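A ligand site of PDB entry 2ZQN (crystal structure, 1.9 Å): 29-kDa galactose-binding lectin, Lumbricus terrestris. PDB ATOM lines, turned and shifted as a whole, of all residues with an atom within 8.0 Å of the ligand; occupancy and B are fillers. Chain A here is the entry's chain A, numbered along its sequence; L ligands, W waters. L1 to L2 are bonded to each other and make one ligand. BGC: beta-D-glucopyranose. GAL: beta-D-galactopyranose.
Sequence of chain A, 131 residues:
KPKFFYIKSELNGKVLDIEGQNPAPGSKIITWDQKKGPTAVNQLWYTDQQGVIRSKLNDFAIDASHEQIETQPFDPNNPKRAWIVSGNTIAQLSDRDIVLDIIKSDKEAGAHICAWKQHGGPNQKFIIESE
An oxygen (O3) of GAL L2 sits at hydrogen-bond distance from the side-chain amide nitrogen of Asn 42. O3 of GAL L2 sits at hydrogen-bond distance from OD2 of Asp 17, at 2.5 Å. The side-chain amino group (NZ) of Lys 35 is in hydrogen-bond range of an oxygen (O2) of GAL L2, 2.8 Å away. N of Gly 20 sits at hydrogen-bond distance from O4 of GAL L2 (2.8 Å).
The backbone carbonyl oxygen (O) of Trp 32 lies within hydrogen-bond range of the backbone NH (N) of Val 15, 2.9 Å away. The backbone carbonyl oxygen (O) of Thr 39 is in hydrogen-bond range of the side-chain amide nitrogen (NE2) of Gln 21, 3.3 Å away. The side-chain amide nitrogen of Gln 21 lies within hydrogen-bond range of the side-chain amide oxygen of Asn 42. NE2 of Gln 43 sits at hydrogen-bond distance from OD2 of Asp 17 (2.9 Å). O of Lys 28 is in hydrogen-bond range of N of Glu 19, 3.0 Å away. OD1 of Asp 17 sits at hydrogen-bond distance from ND2 of Asn 42 (3.1 Å). The side-chain amide nitrogen of Asn 42 sits at hydrogen-bond distance from the backbone carbonyl oxygen of Ile 18 (2.8 Å). The backbone NH (N) of Ile 30 sits at hydrogen-bond distance from the backbone carbonyl oxygen (O) of Asp 17.
Residues that only touch the ligand: Gln 21, Glu 19, Trp 32, Ile 18 and Ile 30. Hydrophobic or aromatic side chains within 4 Å of the ligand: Ile 30 and Trp 32. Nine residues have an atom within 4 Å of the ligand: Asp 17, Ile 18, Glu 19, Gly 20, Gln 21, Ile 30, Trp 32, Lys 35 and Asn 42. The nearest printed residue that does not touch the ligand is Gln 43 (4.2 Å).
Water W1 lies within hydrogen-bond range of O6 of GAL L2 (3.3 Å) and OE2 of Glu 19 (3.4 Å).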
ATOM      1  N   VAL A  15      22.916  -5.657  11.320  1.00  0.00           N
ATOM      2  CA  VAL A  15      23.976  -4.638  11.291  1.00  0.00           C
ATOM      3  C   VAL A  15      23.958  -3.890   9.975  1.00  0.00           C
ATOM      4  O   VAL A  15      23.419  -4.410   8.976  1.00  0.00           O
ATOM      5  CB  VAL A  15      25.381  -5.228  11.565  1.00  0.00           C
ATOM      6  CG1 VAL A  15      25.473  -5.909  12.940  1.00  0.00           C
ATOM      7  CG2 VAL A  15      25.820  -6.173  10.415  1.00  0.00           C
ATOM      8  N   LEU A  16      24.551  -2.684   9.939  1.00  0.00           N
ATOM      9  CA  LEU A  16      24.615  -1.949   8.664  1.00  0.00           C
ATOM     10  C   LEU A  16      25.613  -2.620   7.723  1.00  0.00           C
ATOM     11  O   LEU A  16      26.685  -3.093   8.157  1.00  0.00           O
ATOM     12  CB  LEU A  16      24.912  -0.454   8.866  1.00  0.00           C
ATOM     13  CG  LEU A  16      23.873   0.354   9.643  1.00  0.00           C
ATOM     14  CD1 LEU A  16      24.140   1.831   9.467  1.00  0.00           C
ATOM     15  CD2 LEU A  16      22.432   0.031   9.217  1.00  0.00           C
ATOM     16  N   ASP A  17      25.264  -2.680   6.445  1.00  0.00           N
ATOM     17  CA  ASP A  17      25.921  -3.584   5.492  1.00  0.00           C
ATOM     18  C   ASP A  17      25.853  -2.909   4.115  1.00  0.00           C
ATOM     19  O   ASP A  17      24.793  -2.456   3.710  1.00  0.00           O
ATOM     20  CB  ASP A  17      25.180  -4.930   5.563  1.00  0.00           C
ATOM     21  CG  ASP A  17      25.642  -5.969   4.556  1.00  0.00           C
ATOM     22  OD1 ASP A  17      25.627  -5.673   3.339  1.00  0.00           O
ATOM     23  OD2 ASP A  17      25.939  -7.117   4.979  1.00  0.00           O
ATOM     24  N   ILE A  18      26.980  -2.815   3.412  1.00  0.00           N
ATOM     25  CA  ILE A  18      26.984  -2.360   2.029  1.00  0.00           C
ATOM     26  C   ILE A  18      26.572  -3.550   1.123  1.00  0.00           C
ATOM     27  O   ILE A  18      27.313  -4.551   0.973  1.00  0.00           O
ATOM     28  CB  ILE A  18      28.354  -1.807   1.591  1.00  0.00           C
ATOM     29  CG1 ILE A  18      28.807  -0.659   2.499  1.00  0.00           C
ATOM     30  CG2 ILE A  18      28.284  -1.329   0.138  1.00  0.00           C
ATOM     31  CD1 ILE A  18      30.301  -0.328   2.291  1.00  0.00           C
ATOM     32  N   GLU A  19      25.393  -3.387   0.553  1.00  0.00           N
ATOM     33  CA  GLU A  19      24.706  -4.439  -0.193  1.00  0.00           C
ATOM     34  C   GLU A  19      25.616  -5.146  -1.206  1.00  0.00           C
ATOM     35  O   GLU A  19      26.243  -4.486  -2.046  1.00  0.00           O
ATOM     36  CB  GLU A  19      23.493  -3.833  -0.901  1.00  0.00           C
ATOM     37  CG  GLU A  19      22.743  -4.866  -1.761  1.00  0.00           C
ATOM     38  CD  GLU A  19      21.426  -4.381  -2.301  1.00  0.00           C
ATOM     39  OE1 GLU A  19      21.277  -3.187  -2.595  1.00  0.00           O
ATOM     40  OE2 GLU A  19      20.518  -5.236  -2.445  1.00  0.00           O
ATOM     41  N   GLY A  20      25.734  -6.463  -1.070  1.00  0.00           N
ATOM     42  CA  GLY A  20      26.478  -7.302  -2.033  1.00  0.00           C
ATOM     43  C   GLY A  20      27.986  -7.108  -2.008  1.00  0.00           C
ATOM     44  O   GLY A  20      28.663  -7.505  -2.943  1.00  0.00           O
ATOM     45  N   GLN A  21      28.502  -6.487  -0.949  1.00  0.00           N
ATOM     46  CA  GLN A  21      29.934  -6.193  -0.838  1.00  0.00           C
ATOM     47  C   GLN A  21      30.437  -5.294  -1.982  1.00  0.00           C
ATOM     48  O   GLN A  21      31.642  -5.327  -2.358  1.00  0.00           O
ATOM     49  CB  GLN A  21      30.795  -7.482  -0.738  1.00  0.00           C
ATOM     50  CG  GLN A  21      30.313  -8.514   0.279  1.00  0.00           C
ATOM     51  CD  GLN A  21      31.369  -9.584   0.548  1.00  0.00           C
ATOM     52  OE1 GLN A  21      31.482 -10.551  -0.221  1.00  0.00           O
ATOM     53  NE2 GLN A  21      32.169  -9.406   1.634  1.00  0.00           N
ATOM     54  N   ASN A  22      29.539  -4.460  -2.485  1.00  0.00           N
ATOM     55  CA  ASN A  22      29.790  -3.627  -3.657  1.00  0.00           C
ATOM     56  C   ASN A  22      30.584  -2.371  -3.259  1.00  0.00           C
ATOM     57  O   ASN A  22      30.106  -1.583  -2.456  1.00  0.00           O
ATOM     58  CB  ASN A  22      28.440  -3.271  -4.290  1.00  0.00           C
ATOM     59  CG  ASN A  22      28.577  -2.649  -5.679  1.00  0.00           C
ATOM     60  OD1 ASN A  22      29.659  -2.255  -6.117  1.00  0.00           O
ATOM     61  ND2 ASN A  22      27.459  -2.549  -6.365  1.00  0.00           N
ATOM     62  N   LYS A  28      23.734   0.670  -1.897  1.00  0.00           N
ATOM     63  CA  LYS A  28      22.821   0.923  -0.798  1.00  0.00           C
ATOM     64  C   LYS A  28      23.392   0.361   0.488  1.00  0.00           C
ATOM     65  O   LYS A  28      23.992  -0.723   0.496  1.00  0.00           O
ATOM     66  CB  LYS A  28      21.436   0.258  -1.040  1.00  0.00           C
ATOM     67  CG  LYS A  28      20.739   0.704  -2.290  1.00  0.00           C
ATOM     68  CD  LYS A  28      20.069   2.034  -2.100  1.00  0.00           C
ATOM     69  CE  LYS A  28      19.505   2.525  -3.436  1.00  0.00           C
ATOM     70  NZ  LYS A  28      18.608   3.682  -3.232  1.00  0.00           N
ATOM     71  N   ILE A  30      22.191  -1.318   3.857  1.00  0.00           N
ATOM     72  CA  ILE A  30      20.959  -2.050   4.254  1.00  0.00           C
ATOM     73  C   ILE A  30      21.233  -2.719   5.603  1.00  0.00           C
ATOM     74  O   ILE A  30      22.382  -2.742   6.058  1.00  0.00           O
ATOM     75  CB  ILE A  30      20.618  -3.169   3.193  1.00  0.00           C
ATOM     76  CG1 ILE A  30      21.753  -4.209   3.128  1.00  0.00           C
ATOM     77  CG2 ILE A  30      20.327  -2.535   1.802  1.00  0.00           C
ATOM     78  CD1 ILE A  30      21.505  -5.434   2.187  1.00  0.00           C
ATOM     79  N   THR A  31      20.199  -3.236   6.247  1.00  0.00           N
ATOM     80  CA  THR A  31      20.420  -4.106   7.411  1.00  0.00           C
ATOM     81  C   THR A  31      20.714  -5.519   6.915  1.00  0.00           C
ATOM     82  O   THR A  31      20.169  -5.928   5.888  1.00  0.00           O
ATOM     83  CB  THR A  31      19.212  -4.135   8.335  1.00  0.00           C
ATOM     84  OG1 THR A  31      18.076  -4.625   7.602  1.00  0.00           O
ATOM     85  CG2 THR A  31      18.871  -2.770   8.852  1.00  0.00           C
ATOM     86  N   TRP A  32      21.547  -6.273   7.643  1.00  0.00           N
ATOM     87  CA  TRP A  32      21.826  -7.654   7.245  1.00  0.00           C
ATOM     88  C   TRP A  32      22.308  -8.413   8.459  1.00  0.00           C
ATOM     89  O   TRP A  32      22.839  -7.824   9.420  1.00  0.00           O
ATOM     90  CB  TRP A  32      22.882  -7.690   6.119  1.00  0.00           C
ATOM     91  CG  TRP A  32      22.845  -8.937   5.293  1.00  0.00           C
ATOM     92  CD1 TRP A  32      23.746  -9.971   5.316  1.00  0.00           C
ATOM     93  CD2 TRP A  32      21.822  -9.303   4.356  1.00  0.00           C
ATOM     94  NE1 TRP A  32      23.359 -10.952   4.409  1.00  0.00           N
ATOM     95  CE2 TRP A  32      22.183 -10.573   3.816  1.00  0.00           C
ATOM     96  CE3 TRP A  32      20.653  -8.676   3.892  1.00  0.00           C
ATOM     97  CZ2 TRP A  32      21.405 -11.221   2.846  1.00  0.00           C
ATOM     98  CZ3 TRP A  32      19.861  -9.328   2.922  1.00  0.00           C
ATOM     99  CH2 TRP A  32      20.246 -10.586   2.416  1.00  0.00           C
ATOM    100  N   ASP A  33      22.168  -9.739   8.427  1.00  0.00           N
ATOM    101  CA  ASP A  33      22.663 -10.550   9.531  1.00  0.00           C
ATOM    102  C   ASP A  33      24.174 -10.414   9.633  1.00  0.00           C
ATOM    103  O   ASP A  33      24.884 -10.445   8.617  1.00  0.00           O
ATOM    104  CB  ASP A  33      22.254 -12.019   9.371  1.00  0.00           C
ATOM    105  CG  ASP A  33      20.753 -12.239   9.576  1.00  0.00           C
ATOM    106  OD1 ASP A  33      20.095 -11.433  10.249  1.00  0.00           O
ATOM    107  OD2 ASP A  33      20.237 -13.244   9.074  1.00  0.00           O
ATOM    108  N   GLN A  34      24.652 -10.273  10.862  1.00  0.00           N
ATOM    109  CA  GLN A  34      26.069 -10.042  11.123  1.00  0.00           C
ATOM    110  C   GLN A  34      27.006 -11.190  10.701  1.00  0.00           C
ATOM    111  O   GLN A  34      26.781 -12.387  11.017  1.00  0.00           O
ATOM    112  CB  GLN A  34      26.245  -9.762  12.605  1.00  0.00           C
ATOM    113  CG  GLN A  34      27.664  -9.440  13.026  1.00  0.00           C
ATOM    114  CD  GLN A  34      27.754  -9.046  14.470  1.00  0.00           C
ATOM    115  OE1 GLN A  34      26.979  -9.505  15.323  1.00  0.00           O
ATOM    116  NE2 GLN A  34      28.723  -8.180  14.782  1.00  0.00           N
ATOM    117  N   LYS A  35      28.051 -10.814   9.983  1.00  0.00           N
ATOM    118  CA  LYS A  35      29.136 -11.726   9.609  1.00  0.00           C
ATOM    119  C   LYS A  35      30.304 -11.435  10.534  1.00  0.00           C
ATOM    120  O   LYS A  35      30.476 -10.294  10.947  1.00  0.00           O
ATOM    121  CB  LYS A  35      29.598 -11.437   8.180  1.00  0.00           C
ATOM    122  CG  LYS A  35      28.564 -11.735   7.120  1.00  0.00           C
ATOM    123  CD  LYS A  35      29.156 -11.561   5.738  1.00  0.00           C
ATOM    124  CE  LYS A  35      28.987 -10.135   5.257  1.00  0.00           C
ATOM    125  NZ  LYS A  35      29.604 -10.067   3.917  1.00  0.00           N
ATOM    126  N   THR A  39      35.369 -12.000   5.819  1.00  0.00           N
ATOM    127  CA  THR A  39      34.278 -11.565   4.925  1.00  0.00           C
ATOM    128  C   THR A  39      33.358 -10.489   5.498  1.00  0.00           C
ATOM    129  O   THR A  39      32.405 -10.076   4.825  1.00  0.00           O
ATOM    130  CB  THR A  39      33.389 -12.716   4.431  1.00  0.00           C
ATOM    131  OG1 THR A  39      32.577 -13.201   5.502  1.00  0.00           O
ATOM    132  CG2 THR A  39      34.232 -13.849   3.816  1.00  0.00           C
ATOM    133  N   ALA A  40      33.626 -10.026   6.729  1.00  0.00           N
ATOM    134  CA  ALA A  40      32.810  -8.994   7.346  1.00  0.00           C
ATOM    135  C   ALA A  40      33.129  -7.553   6.849  1.00  0.00           C
ATOM    136  O   ALA A  40      32.568  -6.604   7.362  1.00  0.00           O
ATOM    137  CB  ALA A  40      32.931  -9.034   8.834  1.00  0.00           C
ATOM    138  N   VAL A  41      34.043  -7.428   5.888  1.00  0.00           N
ATOM    139  CA  VAL A  41      34.582  -6.120   5.486  1.00  0.00           C
ATOM    140  C   VAL A  41      33.508  -5.050   5.163  1.00  0.00           C
ATOM    141  O   VAL A  41      33.651  -3.881   5.561  1.00  0.00           O
ATOM    142  CB  VAL A  41      35.624  -6.267   4.334  1.00  0.00           C
ATOM    143  CG1 VAL A  41      34.959  -6.829   3.062  1.00  0.00           C
ATOM    144  CG2 VAL A  41      36.351  -4.927   4.066  1.00  0.00           C
ATOM    145  N   ASN A  42      32.436  -5.456   4.451  1.00  0.00           N
ATOM    146  CA  ASN A  42      31.335  -4.549   4.084  1.00  0.00           C
ATOM    147  C   ASN A  42      30.323  -4.328   5.242  1.00  0.00           C
ATOM    148  O   ASN A  42      29.324  -3.655   5.047  1.00  0.00           O
ATOM    149  CB  ASN A  42      30.585  -5.043   2.819  1.00  0.00           C
ATOM    150  CG  ASN A  42      29.852  -6.350   3.062  1.00  0.00           C
ATOM    151  OD1 ASN A  42      30.443  -7.319   3.532  1.00  0.00           O
ATOM    152  ND2 ASN A  42      28.543  -6.386   2.707  1.00  0.00           N
ATOM    153  N   GLN A  43      30.581  -4.895   6.419  1.00  0.00           N
ATOM    154  CA  GLN A  43      29.816  -4.531   7.614  1.00  0.00           C
ATOM    155  C   GLN A  43      30.657  -3.776   8.650  1.00  0.00           C
ATOM    156  O   GLN A  43      30.175  -3.494   9.759  1.00  0.00           O
ATOM    157  CB  GLN A  43      29.200  -5.774   8.274  1.00  0.00           C
ATOM    158  CG  GLN A  43      28.339  -6.623   7.347  1.00  0.00           C
ATOM    159  CD  GLN A  43      27.725  -7.823   8.040  1.00  0.00           C
ATOM    160  OE1 GLN A  43      28.244  -8.293   9.079  1.00  0.00           O
ATOM    161  NE2 GLN A  43      26.608  -8.294   7.509  1.00  0.00           N
ATOM    162  N   ALA A 109      15.678  -8.662   7.067  1.00  0.00           N
ATOM    163  CA  ALA A 109      17.025  -8.438   6.501  1.00  0.00           C
ATOM    164  C   ALA A 109      16.901  -7.772   5.128  1.00  0.00           C
ATOM    165  O   ALA A 109      15.956  -8.038   4.377  1.00  0.00           O
ATOM    166  CB  ALA A 109      17.798  -9.734   6.399  1.00  0.00           C
ATOM    167  N   GLY A 110      17.827  -6.874   4.816  1.00  0.00           N
ATOM    168  CA  GLY A 110      17.769  -6.153   3.546  1.00  0.00           C
ATOM    169  C   GLY A 110      16.975  -4.869   3.589  1.00  0.00           C
ATOM    170  O   GLY A 110      16.753  -4.250   2.546  1.00  0.00           O
HETATM  171  C2  BGC L   1      25.360 -12.583  -3.830  1.00  0.00           C
HETATM  172  C3  BGC L   1      25.647 -11.420  -2.899  1.00  0.00           C
HETATM  173  C4  BGC L   1      26.466 -11.851  -1.678  1.00  0.00           C
HETATM  174  C5  BGC L   1      27.692 -12.708  -2.079  1.00  0.00           C
HETATM  175  C6  BGC L   1      28.380 -13.359  -0.877  1.00  0.00           C
HETATM  176  C1  BGC L   1      26.666 -13.311  -4.176  1.00  0.00           C
HETATM  177  O1  BGC L   1      26.415 -14.471  -4.990  1.00  0.00           O
HETATM  178  O2  BGC L   1      24.643 -12.088  -4.958  1.00  0.00           O
HETATM  179  O3  BGC L   1      24.404 -10.919  -2.480  1.00  0.00           O
HETATM  180  O4  BGC L   1      26.866 -10.707  -0.940  1.00  0.00           O
HETATM  181  O5  BGC L   1      27.307 -13.754  -2.979  1.00  0.00           O
HETATM  182  O6  BGC L   1      27.503 -14.187  -0.131  1.00  0.00           O
HETATM  183  C1  GAL L   2      26.079 -10.504   0.223  1.00  0.00           C
HETATM  184  C2  GAL L   2      26.971  -9.802   1.257  1.00  0.00           C
HETATM  185  C3  GAL L   2      26.153  -9.445   2.494  1.00  0.00           C
HETATM  186  C4  GAL L   2      24.915  -8.657   2.114  1.00  0.00           C
HETATM  187  C5  GAL L   2      24.105  -9.476   1.080  1.00  0.00           C
HETATM  188  C6  GAL L   2      22.870  -8.711   0.629  1.00  0.00           C
HETATM  189  O2  GAL L   2      28.030 -10.661   1.631  1.00  0.00           O
HETATM  190  O3  GAL L   2      26.977  -8.696   3.381  1.00  0.00           O
HETATM  191  O4  GAL L   2      25.319  -7.410   1.547  1.00  0.00           O
HETATM  192  O5  GAL L   2      24.931  -9.722  -0.058  1.00  0.00           O
HETATM  193  O6  GAL L   2      22.255  -9.390  -0.478  1.00  0.00           O
HETATM  194  O   HOH W   1      19.280  -7.947  -0.801  1.00  0.00           O
HETATM  195  O   HOH W   2      25.391 -15.733  -0.949  1.00  0.00           O
HETATM  196  O   HOH W   3      29.413 -14.313   2.603  1.00  0.00           O
HETATM  197  O   HOH W   4      21.725 -12.009  -0.772  1.00  0.00           O
HETATM  198  O   HOH W   5      22.197 -11.178  -4.136  1.00  0.00           O
